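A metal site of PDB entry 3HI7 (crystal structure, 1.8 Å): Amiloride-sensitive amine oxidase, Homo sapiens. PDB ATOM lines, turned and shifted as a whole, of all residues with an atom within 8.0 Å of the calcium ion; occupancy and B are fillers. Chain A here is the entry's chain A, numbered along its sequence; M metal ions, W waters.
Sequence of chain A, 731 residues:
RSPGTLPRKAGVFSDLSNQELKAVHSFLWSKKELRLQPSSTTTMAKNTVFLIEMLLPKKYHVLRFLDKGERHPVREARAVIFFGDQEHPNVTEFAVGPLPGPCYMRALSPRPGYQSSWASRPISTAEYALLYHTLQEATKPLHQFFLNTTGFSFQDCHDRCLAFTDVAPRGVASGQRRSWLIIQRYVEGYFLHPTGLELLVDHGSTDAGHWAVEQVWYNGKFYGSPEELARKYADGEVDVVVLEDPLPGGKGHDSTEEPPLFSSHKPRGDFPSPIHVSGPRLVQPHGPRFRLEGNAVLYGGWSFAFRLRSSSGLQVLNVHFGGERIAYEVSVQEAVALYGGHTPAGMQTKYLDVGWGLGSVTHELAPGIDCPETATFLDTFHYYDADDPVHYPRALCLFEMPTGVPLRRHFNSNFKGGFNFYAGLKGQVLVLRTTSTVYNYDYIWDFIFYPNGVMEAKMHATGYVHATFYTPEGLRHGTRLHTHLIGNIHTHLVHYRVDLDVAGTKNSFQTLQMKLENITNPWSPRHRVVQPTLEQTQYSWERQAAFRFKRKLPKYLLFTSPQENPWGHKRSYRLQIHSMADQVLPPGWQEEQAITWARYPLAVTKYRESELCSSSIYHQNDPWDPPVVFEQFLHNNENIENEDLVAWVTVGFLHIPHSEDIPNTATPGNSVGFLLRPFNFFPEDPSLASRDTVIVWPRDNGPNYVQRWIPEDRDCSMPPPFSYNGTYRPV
The calcium ion is bound by O of Phe 633 (2.3 Å), OE1 of Glu 638 (2.4 Å), water W1 (2.4 Å), water W2 (2.4 Å), OD1 of Asn 636 (2.4 Å), OE2 of Glu 542 (2.5 Å) and OE1 of Glu 542 (2.5 Å). The calcium ion has seven donor atoms within binding distance.
Within 4 Å of the calcium ion: Glu 542, Phe 633, Asn 636 and Glu 638. Along chain A the residues within 4 Å of the calcium ion span positions 542 to 638. The nearest printed residue that does not touch the calcium ion is Arg 608 (4.02 Å).
Water W2 lies within hydrogen-bond range of OE2 of Glu 611, ND2 of Asn 636 and NH1 of Arg 608. Water W1 lies within hydrogen-bond range of OE1 of Glu 611 (2.6 Å), O of Lys 606 (2.9 Å) and NH1 of Arg 608 (3.2 Å).
The guanidinium group (NH2) of Arg 608 lies within salt-bridge range of the side-chain carboxylate (OE2) of Glu 638, at 2.8 Å. The backbone NH (N) of Lys 606 sits close to the side-chain carboxylate (OE2) of Glu 542, at 2.9 Å. The backbone NH (N) of Glu 542 lies within hydrogen-bond range of the side-chain amide oxygen (OD1) of Asn 637, at 3.3 Å.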
ATOM      1  N   GLU A 542     -16.454   4.217  -7.350  1.00  0.00           N
ATOM      2  CA  GLU A 542     -17.850   4.027  -6.899  1.00  0.00           C
ATOM      3  C   GLU A 542     -18.613   3.023  -7.729  1.00  0.00           C
ATOM      4  O   GLU A 542     -19.277   2.153  -7.189  1.00  0.00           O
ATOM      5  CB  GLU A 542     -18.624   5.345  -6.881  1.00  0.00           C
ATOM      6  CG  GLU A 542     -18.245   6.300  -5.768  1.00  0.00           C
ATOM      7  CD  GLU A 542     -18.874   7.688  -5.923  1.00  0.00           C
ATOM      8  OE1 GLU A 542     -18.978   8.200  -7.060  1.00  0.00           O
ATOM      9  OE2 GLU A 542     -19.300   8.289  -4.885  1.00  0.00           O
ATOM     10  N   ARG A 543     -18.529   3.117  -9.065  1.00  0.00           N
ATOM     11  CA  ARG A 543     -19.309   2.218  -9.926  1.00  0.00           C
ATOM     12  C   ARG A 543     -19.031   0.744  -9.669  1.00  0.00           C
ATOM     13  O   ARG A 543     -19.922  -0.121  -9.830  1.00  0.00           O
ATOM     14  CB  ARG A 543     -19.059   2.544 -11.409  1.00  0.00           C
ATOM     15  CG  ARG A 543     -19.614   3.890 -11.836  1.00  0.00           C
ATOM     16  CD  ARG A 543     -21.110   3.829 -12.032  1.00  0.00           C
ATOM     17  NE  ARG A 543     -21.608   4.992 -12.767  1.00  0.00           N
ATOM     18  CZ  ARG A 543     -22.902   5.255 -12.979  1.00  0.00           C
ATOM     19  NH1 ARG A 543     -23.838   4.466 -12.482  1.00  0.00           N
ATOM     20  NH2 ARG A 543     -23.268   6.320 -13.671  1.00  0.00           N
ATOM     21  N   VAL A 604     -21.945   2.216  -2.640  1.00  0.00           N
ATOM     22  CA  VAL A 604     -20.978   2.897  -1.800  1.00  0.00           C
ATOM     23  C   VAL A 604     -20.660   4.244  -2.444  1.00  0.00           C
ATOM     24  O   VAL A 604     -20.266   4.285  -3.610  1.00  0.00           O
ATOM     25  CB  VAL A 604     -19.717   2.083  -1.597  1.00  0.00           C
ATOM     26  CG1 VAL A 604     -18.690   2.839  -0.725  1.00  0.00           C
ATOM     27  CG2 VAL A 604     -20.038   0.706  -0.976  1.00  0.00           C
ATOM     28  N   THR A 605     -20.850   5.327  -1.708  1.00  0.00           N
ATOM     29  CA  THR A 605     -20.483   6.647  -2.225  1.00  0.00           C
ATOM     30  C   THR A 605     -19.421   7.366  -1.397  1.00  0.00           C
ATOM     31  O   THR A 605     -19.201   7.055  -0.194  1.00  0.00           O
ATOM     32  CB  THR A 605     -21.719   7.574  -2.404  1.00  0.00           C
ATOM     33  OG1 THR A 605     -22.305   7.900  -1.116  1.00  0.00           O
ATOM     34  CG2 THR A 605     -22.779   6.926  -3.279  1.00  0.00           C
ATOM     35  N   LYS A 606     -18.731   8.306  -2.041  1.00  0.00           N
ATOM     36  CA  LYS A 606     -17.898   9.280  -1.328  1.00  0.00           C
ATOM     37  C   LYS A 606     -18.787  10.301  -0.598  1.00  0.00           C
ATOM     38  O   LYS A 606     -19.710  10.877  -1.187  1.00  0.00           O
ATOM     39  CB  LYS A 606     -16.943   9.968  -2.305  1.00  0.00           C
ATOM     40  CG  LYS A 606     -16.098  11.059  -1.655  1.00  0.00           C
ATOM     41  CD  LYS A 606     -14.967  11.490  -2.565  1.00  0.00           C
ATOM     42  CE  LYS A 606     -14.271  12.713  -2.044  1.00  0.00           C
ATOM     43  NZ  LYS A 606     -13.010  12.952  -2.823  1.00  0.00           N
ATOM     44  N   TYR A 607     -18.492  10.506   0.697  1.00  0.00           N
ATOM     45  CA  TYR A 607     -19.241  11.416   1.555  1.00  0.00           C
ATOM     46  C   TYR A 607     -19.244  12.827   0.967  1.00  0.00           C
ATOM     47  O   TYR A 607     -18.194  13.335   0.559  1.00  0.00           O
ATOM     48  CB  TYR A 607     -18.642  11.474   2.971  1.00  0.00           C
ATOM     49  CG  TYR A 607     -19.418  12.400   3.884  1.00  0.00           C
ATOM     50  CD1 TYR A 607     -19.202  13.783   3.859  1.00  0.00           C
ATOM     51  CD2 TYR A 607     -20.397  11.917   4.742  1.00  0.00           C
ATOM     52  CE1 TYR A 607     -19.953  14.649   4.650  1.00  0.00           C
ATOM     53  CE2 TYR A 607     -21.146  12.770   5.533  1.00  0.00           C
ATOM     54  CZ  TYR A 607     -20.927  14.132   5.486  1.00  0.00           C
ATOM     55  OH  TYR A 607     -21.679  14.954   6.306  1.00  0.00           O
ATOM     56  N   ARG A 608     -20.413  13.470   1.010  1.00  0.00           N
ATOM     57  CA  ARG A 608     -20.583  14.843   0.581  1.00  0.00           C
ATOM     58  C   ARG A 608     -21.789  15.462   1.310  1.00  0.00           C
ATOM     59  O   ARG A 608     -22.839  14.826   1.450  1.00  0.00           O
ATOM     60  CB  ARG A 608     -20.734  14.823  -0.955  1.00  0.00           C
ATOM     61  CG  ARG A 608     -21.171  16.026  -1.617  1.00  0.00           C
ATOM     62  CD  ARG A 608     -20.813  15.983  -3.090  1.00  0.00           C
ATOM     63  NE  ARG A 608     -19.375  15.834  -3.277  1.00  0.00           N
ATOM     64  CZ  ARG A 608     -18.775  14.767  -3.790  1.00  0.00           C
ATOM     65  NH1 ARG A 608     -19.485  13.742  -4.231  1.00  0.00           N
ATOM     66  NH2 ARG A 608     -17.457  14.718  -3.861  1.00  0.00           N
ATOM     67  N   GLU A 611     -25.176  15.368  -0.403  1.00  0.00           N
ATOM     68  CA  GLU A 611     -25.723  14.034  -0.679  1.00  0.00           C
ATOM     69  C   GLU A 611     -26.051  13.300   0.633  1.00  0.00           C
ATOM     70  O   GLU A 611     -25.796  12.103   0.774  1.00  0.00           O
ATOM     71  CB  GLU A 611     -24.701  13.210  -1.474  1.00  0.00           C
ATOM     72  CG  GLU A 611     -24.258  13.857  -2.789  1.00  0.00           C
ATOM     73  CD  GLU A 611     -23.250  13.022  -3.557  1.00  0.00           C
ATOM     74  OE1 GLU A 611     -22.909  11.889  -3.116  1.00  0.00           O
ATOM     75  OE2 GLU A 611     -22.742  13.543  -4.590  1.00  0.00           O
ATOM     76  N   PHE A 630     -30.840   9.365  -6.584  1.00  0.00           N
ATOM     77  CA  PHE A 630     -29.696   8.663  -5.981  1.00  0.00           C
ATOM     78  C   PHE A 630     -28.661   8.273  -7.028  1.00  0.00           C
ATOM     79  O   PHE A 630     -27.460   8.367  -6.769  1.00  0.00           O
ATOM     80  CB  PHE A 630     -30.153   7.413  -5.204  1.00  0.00           C
ATOM     81  CG  PHE A 630     -29.016   6.646  -4.617  1.00  0.00           C
ATOM     82  CD1 PHE A 630     -28.478   7.003  -3.399  1.00  0.00           C
ATOM     83  CD2 PHE A 630     -28.452   5.572  -5.308  1.00  0.00           C
ATOM     84  CE1 PHE A 630     -27.397   6.326  -2.875  1.00  0.00           C
ATOM     85  CE2 PHE A 630     -27.393   4.885  -4.780  1.00  0.00           C
ATOM     86  CZ  PHE A 630     -26.852   5.257  -3.581  1.00  0.00           C
ATOM     87  N   GLU A 631     -29.120   7.851  -8.196  1.00  0.00           N
ATOM     88  CA  GLU A 631     -28.211   7.446  -9.290  1.00  0.00           C
ATOM     89  C   GLU A 631     -27.180   8.511  -9.620  1.00  0.00           C
ATOM     90  O   GLU A 631     -26.039   8.194  -9.965  1.00  0.00           O
ATOM     91  CB  GLU A 631     -29.021   7.069 -10.536  1.00  0.00           C
ATOM     92  CG  GLU A 631     -28.175   6.609 -11.736  1.00  0.00           C
ATOM     93  CD  GLU A 631     -27.604   5.217 -11.557  1.00  0.00           C
ATOM     94  OE1 GLU A 631     -27.953   4.517 -10.572  1.00  0.00           O
ATOM     95  OE2 GLU A 631     -26.796   4.800 -12.431  1.00  0.00           O
ATOM     96  N   GLN A 632     -27.573   9.783  -9.494  1.00  0.00           N
ATOM     97  CA  GLN A 632     -26.695  10.899  -9.719  1.00  0.00           C
ATOM     98  C   GLN A 632     -25.474  10.928  -8.812  1.00  0.00           C
ATOM     99  O   GLN A 632     -24.440  11.426  -9.235  1.00  0.00           O
ATOM    100  CB  GLN A 632     -27.455  12.248  -9.663  1.00  0.00           C
ATOM    101  CG  GLN A 632     -28.439  12.421 -10.834  1.00  0.00           C
ATOM    102  CD  GLN A 632     -29.294  13.681 -10.759  1.00  0.00           C
ATOM    103  OE1 GLN A 632     -29.138  14.532  -9.863  1.00  0.00           O
ATOM    104  NE2 GLN A 632     -30.230  13.804 -11.710  1.00  0.00           N
ATOM    105  N   PHE A 633     -25.553  10.347  -7.596  1.00  0.00           N
ATOM    106  CA  PHE A 633     -24.403  10.292  -6.704  1.00  0.00           C
ATOM    107  C   PHE A 633     -23.301   9.359  -7.273  1.00  0.00           C
ATOM    108  O   PHE A 633     -22.128   9.433  -6.857  1.00  0.00           O
ATOM    109  CB  PHE A 633     -24.796   9.733  -5.327  1.00  0.00           C
ATOM    110  CG  PHE A 633     -25.869  10.491  -4.573  1.00  0.00           C
ATOM    111  CD1 PHE A 633     -26.413  11.696  -5.005  1.00  0.00           C
ATOM    112  CD2 PHE A 633     -26.318   9.959  -3.356  1.00  0.00           C
ATOM    113  CE1 PHE A 633     -27.434  12.319  -4.243  1.00  0.00           C
ATOM    114  CE2 PHE A 633     -27.283  10.571  -2.600  1.00  0.00           C
ATOM    115  CZ  PHE A 633     -27.829  11.775  -3.022  1.00  0.00           C
ATOM    116  N   LEU A 634     -23.687   8.453  -8.166  1.00  0.00           N
ATOM    117  CA  LEU A 634     -22.761   7.524  -8.827  1.00  0.00           C
ATOM    118  C   LEU A 634     -22.240   8.027 -10.170  1.00  0.00           C
ATOM    119  O   LEU A 634     -21.258   7.510 -10.666  1.00  0.00           O
ATOM    120  CB  LEU A 634     -23.419   6.163  -9.043  1.00  0.00           C
ATOM    121  CG  LEU A 634     -24.069   5.515  -7.808  1.00  0.00           C
ATOM    122  CD1 LEU A 634     -24.836   4.257  -8.195  1.00  0.00           C
ATOM    123  CD2 LEU A 634     -22.965   5.235  -6.775  1.00  0.00           C
ATOM    124  N   HIS A 635     -22.870   9.044 -10.752  1.00  0.00           N
ATOM    125  CA  HIS A 635     -22.462   9.541 -12.065  1.00  0.00           C
ATOM    126  C   HIS A 635     -20.976   9.890 -12.158  1.00  0.00           C
ATOM    127  O   HIS A 635     -20.320   9.582 -13.165  1.00  0.00           O
ATOM    128  CB  HIS A 635     -23.283  10.774 -12.462  1.00  0.00           C
ATOM    129  CG  HIS A 635     -24.664  10.448 -12.931  1.00  0.00           C
ATOM    130  ND1 HIS A 635     -25.611  11.413 -13.150  1.00  0.00           N
ATOM    131  CD2 HIS A 635     -25.244   9.267 -13.239  1.00  0.00           C
ATOM    132  CE1 HIS A 635     -26.728  10.839 -13.578  1.00  0.00           C
ATOM    133  NE2 HIS A 635     -26.517   9.541 -13.654  1.00  0.00           N
ATOM    134  N   ASN A 636     -20.433  10.536 -11.131  1.00  0.00           N
ATOM    135  CA  ASN A 636     -19.044  10.938 -11.186  1.00  0.00           C
ATOM    136  C   ASN A 636     -18.019   9.865 -10.837  1.00  0.00           C
ATOM    137  O   ASN A 636     -16.819  10.111 -10.893  1.00  0.00           O
ATOM    138  CB  ASN A 636     -18.767  12.228 -10.407  1.00  0.00           C
ATOM    139  CG  ASN A 636     -19.127  12.149  -8.931  1.00  0.00           C
ATOM    140  OD1 ASN A 636     -19.459  11.087  -8.410  1.00  0.00           O
ATOM    141  ND2 ASN A 636     -19.064  13.299  -8.253  1.00  0.00           N
ATOM    142  N   ASN A 637     -18.488   8.657 -10.499  1.00  0.00           N
ATOM    143  CA  ASN A 637     -17.615   7.492 -10.365  1.00  0.00           C
ATOM    144  C   ASN A 637     -16.309   7.775  -9.617  1.00  0.00           C
ATOM    145  O   ASN A 637     -15.187   7.549 -10.130  1.00  0.00           O
ATOM    146  CB  ASN A 637     -17.315   6.849 -11.733  1.00  0.00           C
ATOM    147  CG  ASN A 637     -16.742   5.450 -11.585  1.00  0.00           C
ATOM    148  OD1 ASN A 637     -16.916   4.817 -10.546  1.00  0.00           O
ATOM    149  ND2 ASN A 637     -16.029   4.952 -12.617  1.00  0.00           N
ATOM    150  N   GLU A 638     -16.454   8.267  -8.401  1.00  0.00           N
ATOM    151  CA  GLU A 638     -15.330   8.783  -7.661  1.00  0.00           C
ATOM    152  C   GLU A 638     -14.423   7.709  -7.096  1.00  0.00           C
ATOM    153  O   GLU A 638     -14.845   6.575  -6.834  1.00  0.00           O
ATOM    154  CB  GLU A 638     -15.804   9.727  -6.545  1.00  0.00           C
ATOM    155  CG  GLU A 638     -16.382  11.012  -7.108  1.00  0.00           C
ATOM    156  CD  GLU A 638     -16.998  11.851  -6.029  1.00  0.00           C
ATOM    157  OE1 GLU A 638     -18.123  11.523  -5.601  1.00  0.00           O
ATOM    158  OE2 GLU A 638     -16.357  12.849  -5.641  1.00  0.00           O
ATOM    159  N   ASN A 639     -13.162   8.065  -6.919  1.00  0.00           N
ATOM    160  CA  ASN A 639     -12.232   7.181  -6.243  1.00  0.00           C
ATOM    161  C   ASN A 639     -12.663   6.960  -4.795  1.00  0.00           C
ATOM    162  O   ASN A 639     -13.025   7.911  -4.105  1.00  0.00           O
ATOM    163  CB  ASN A 639     -10.803   7.713  -6.331  1.00  0.00           C
ATOM    164  CG  ASN A 639      -9.787   6.673  -5.899  1.00  0.00           C
ATOM    165  OD1 ASN A 639      -9.593   6.480  -4.707  1.00  0.00           O
ATOM    166  ND2 ASN A 639      -9.193   5.930  -6.864  1.00  0.00           N
ATOM    167  N   ILE A 640     -12.679   5.697  -4.361  1.00  0.00           N
ATOM    168  CA  ILE A 640     -13.137   5.320  -3.003  1.00  0.00           C
ATOM    169  C   ILE A 640     -12.046   4.551  -2.232  1.00  0.00           C
ATOM    170  O   ILE A 640     -12.342   3.788  -1.287  1.00  0.00           O
ATOM    171  CB  ILE A 640     -14.458   4.535  -3.023  1.00  0.00           C
ATOM    172  CG1 ILE A 640     -14.335   3.275  -3.904  1.00  0.00           C
ATOM    173  CG2 ILE A 640     -15.628   5.475  -3.433  1.00  0.00           C
ATOM    174  CD1 ILE A 640     -15.437   2.220  -3.720  1.00  0.00           C
HETATM  175 CA    CA M   1     -20.067  10.277  -6.192  1.00  0.00          CA
HETATM  176  O   HOH W   1     -20.690  10.785  -3.914  1.00  0.00           O
HETATM  177  O   HOH W   2     -21.268  12.367  -6.461  1.00  0.00           O
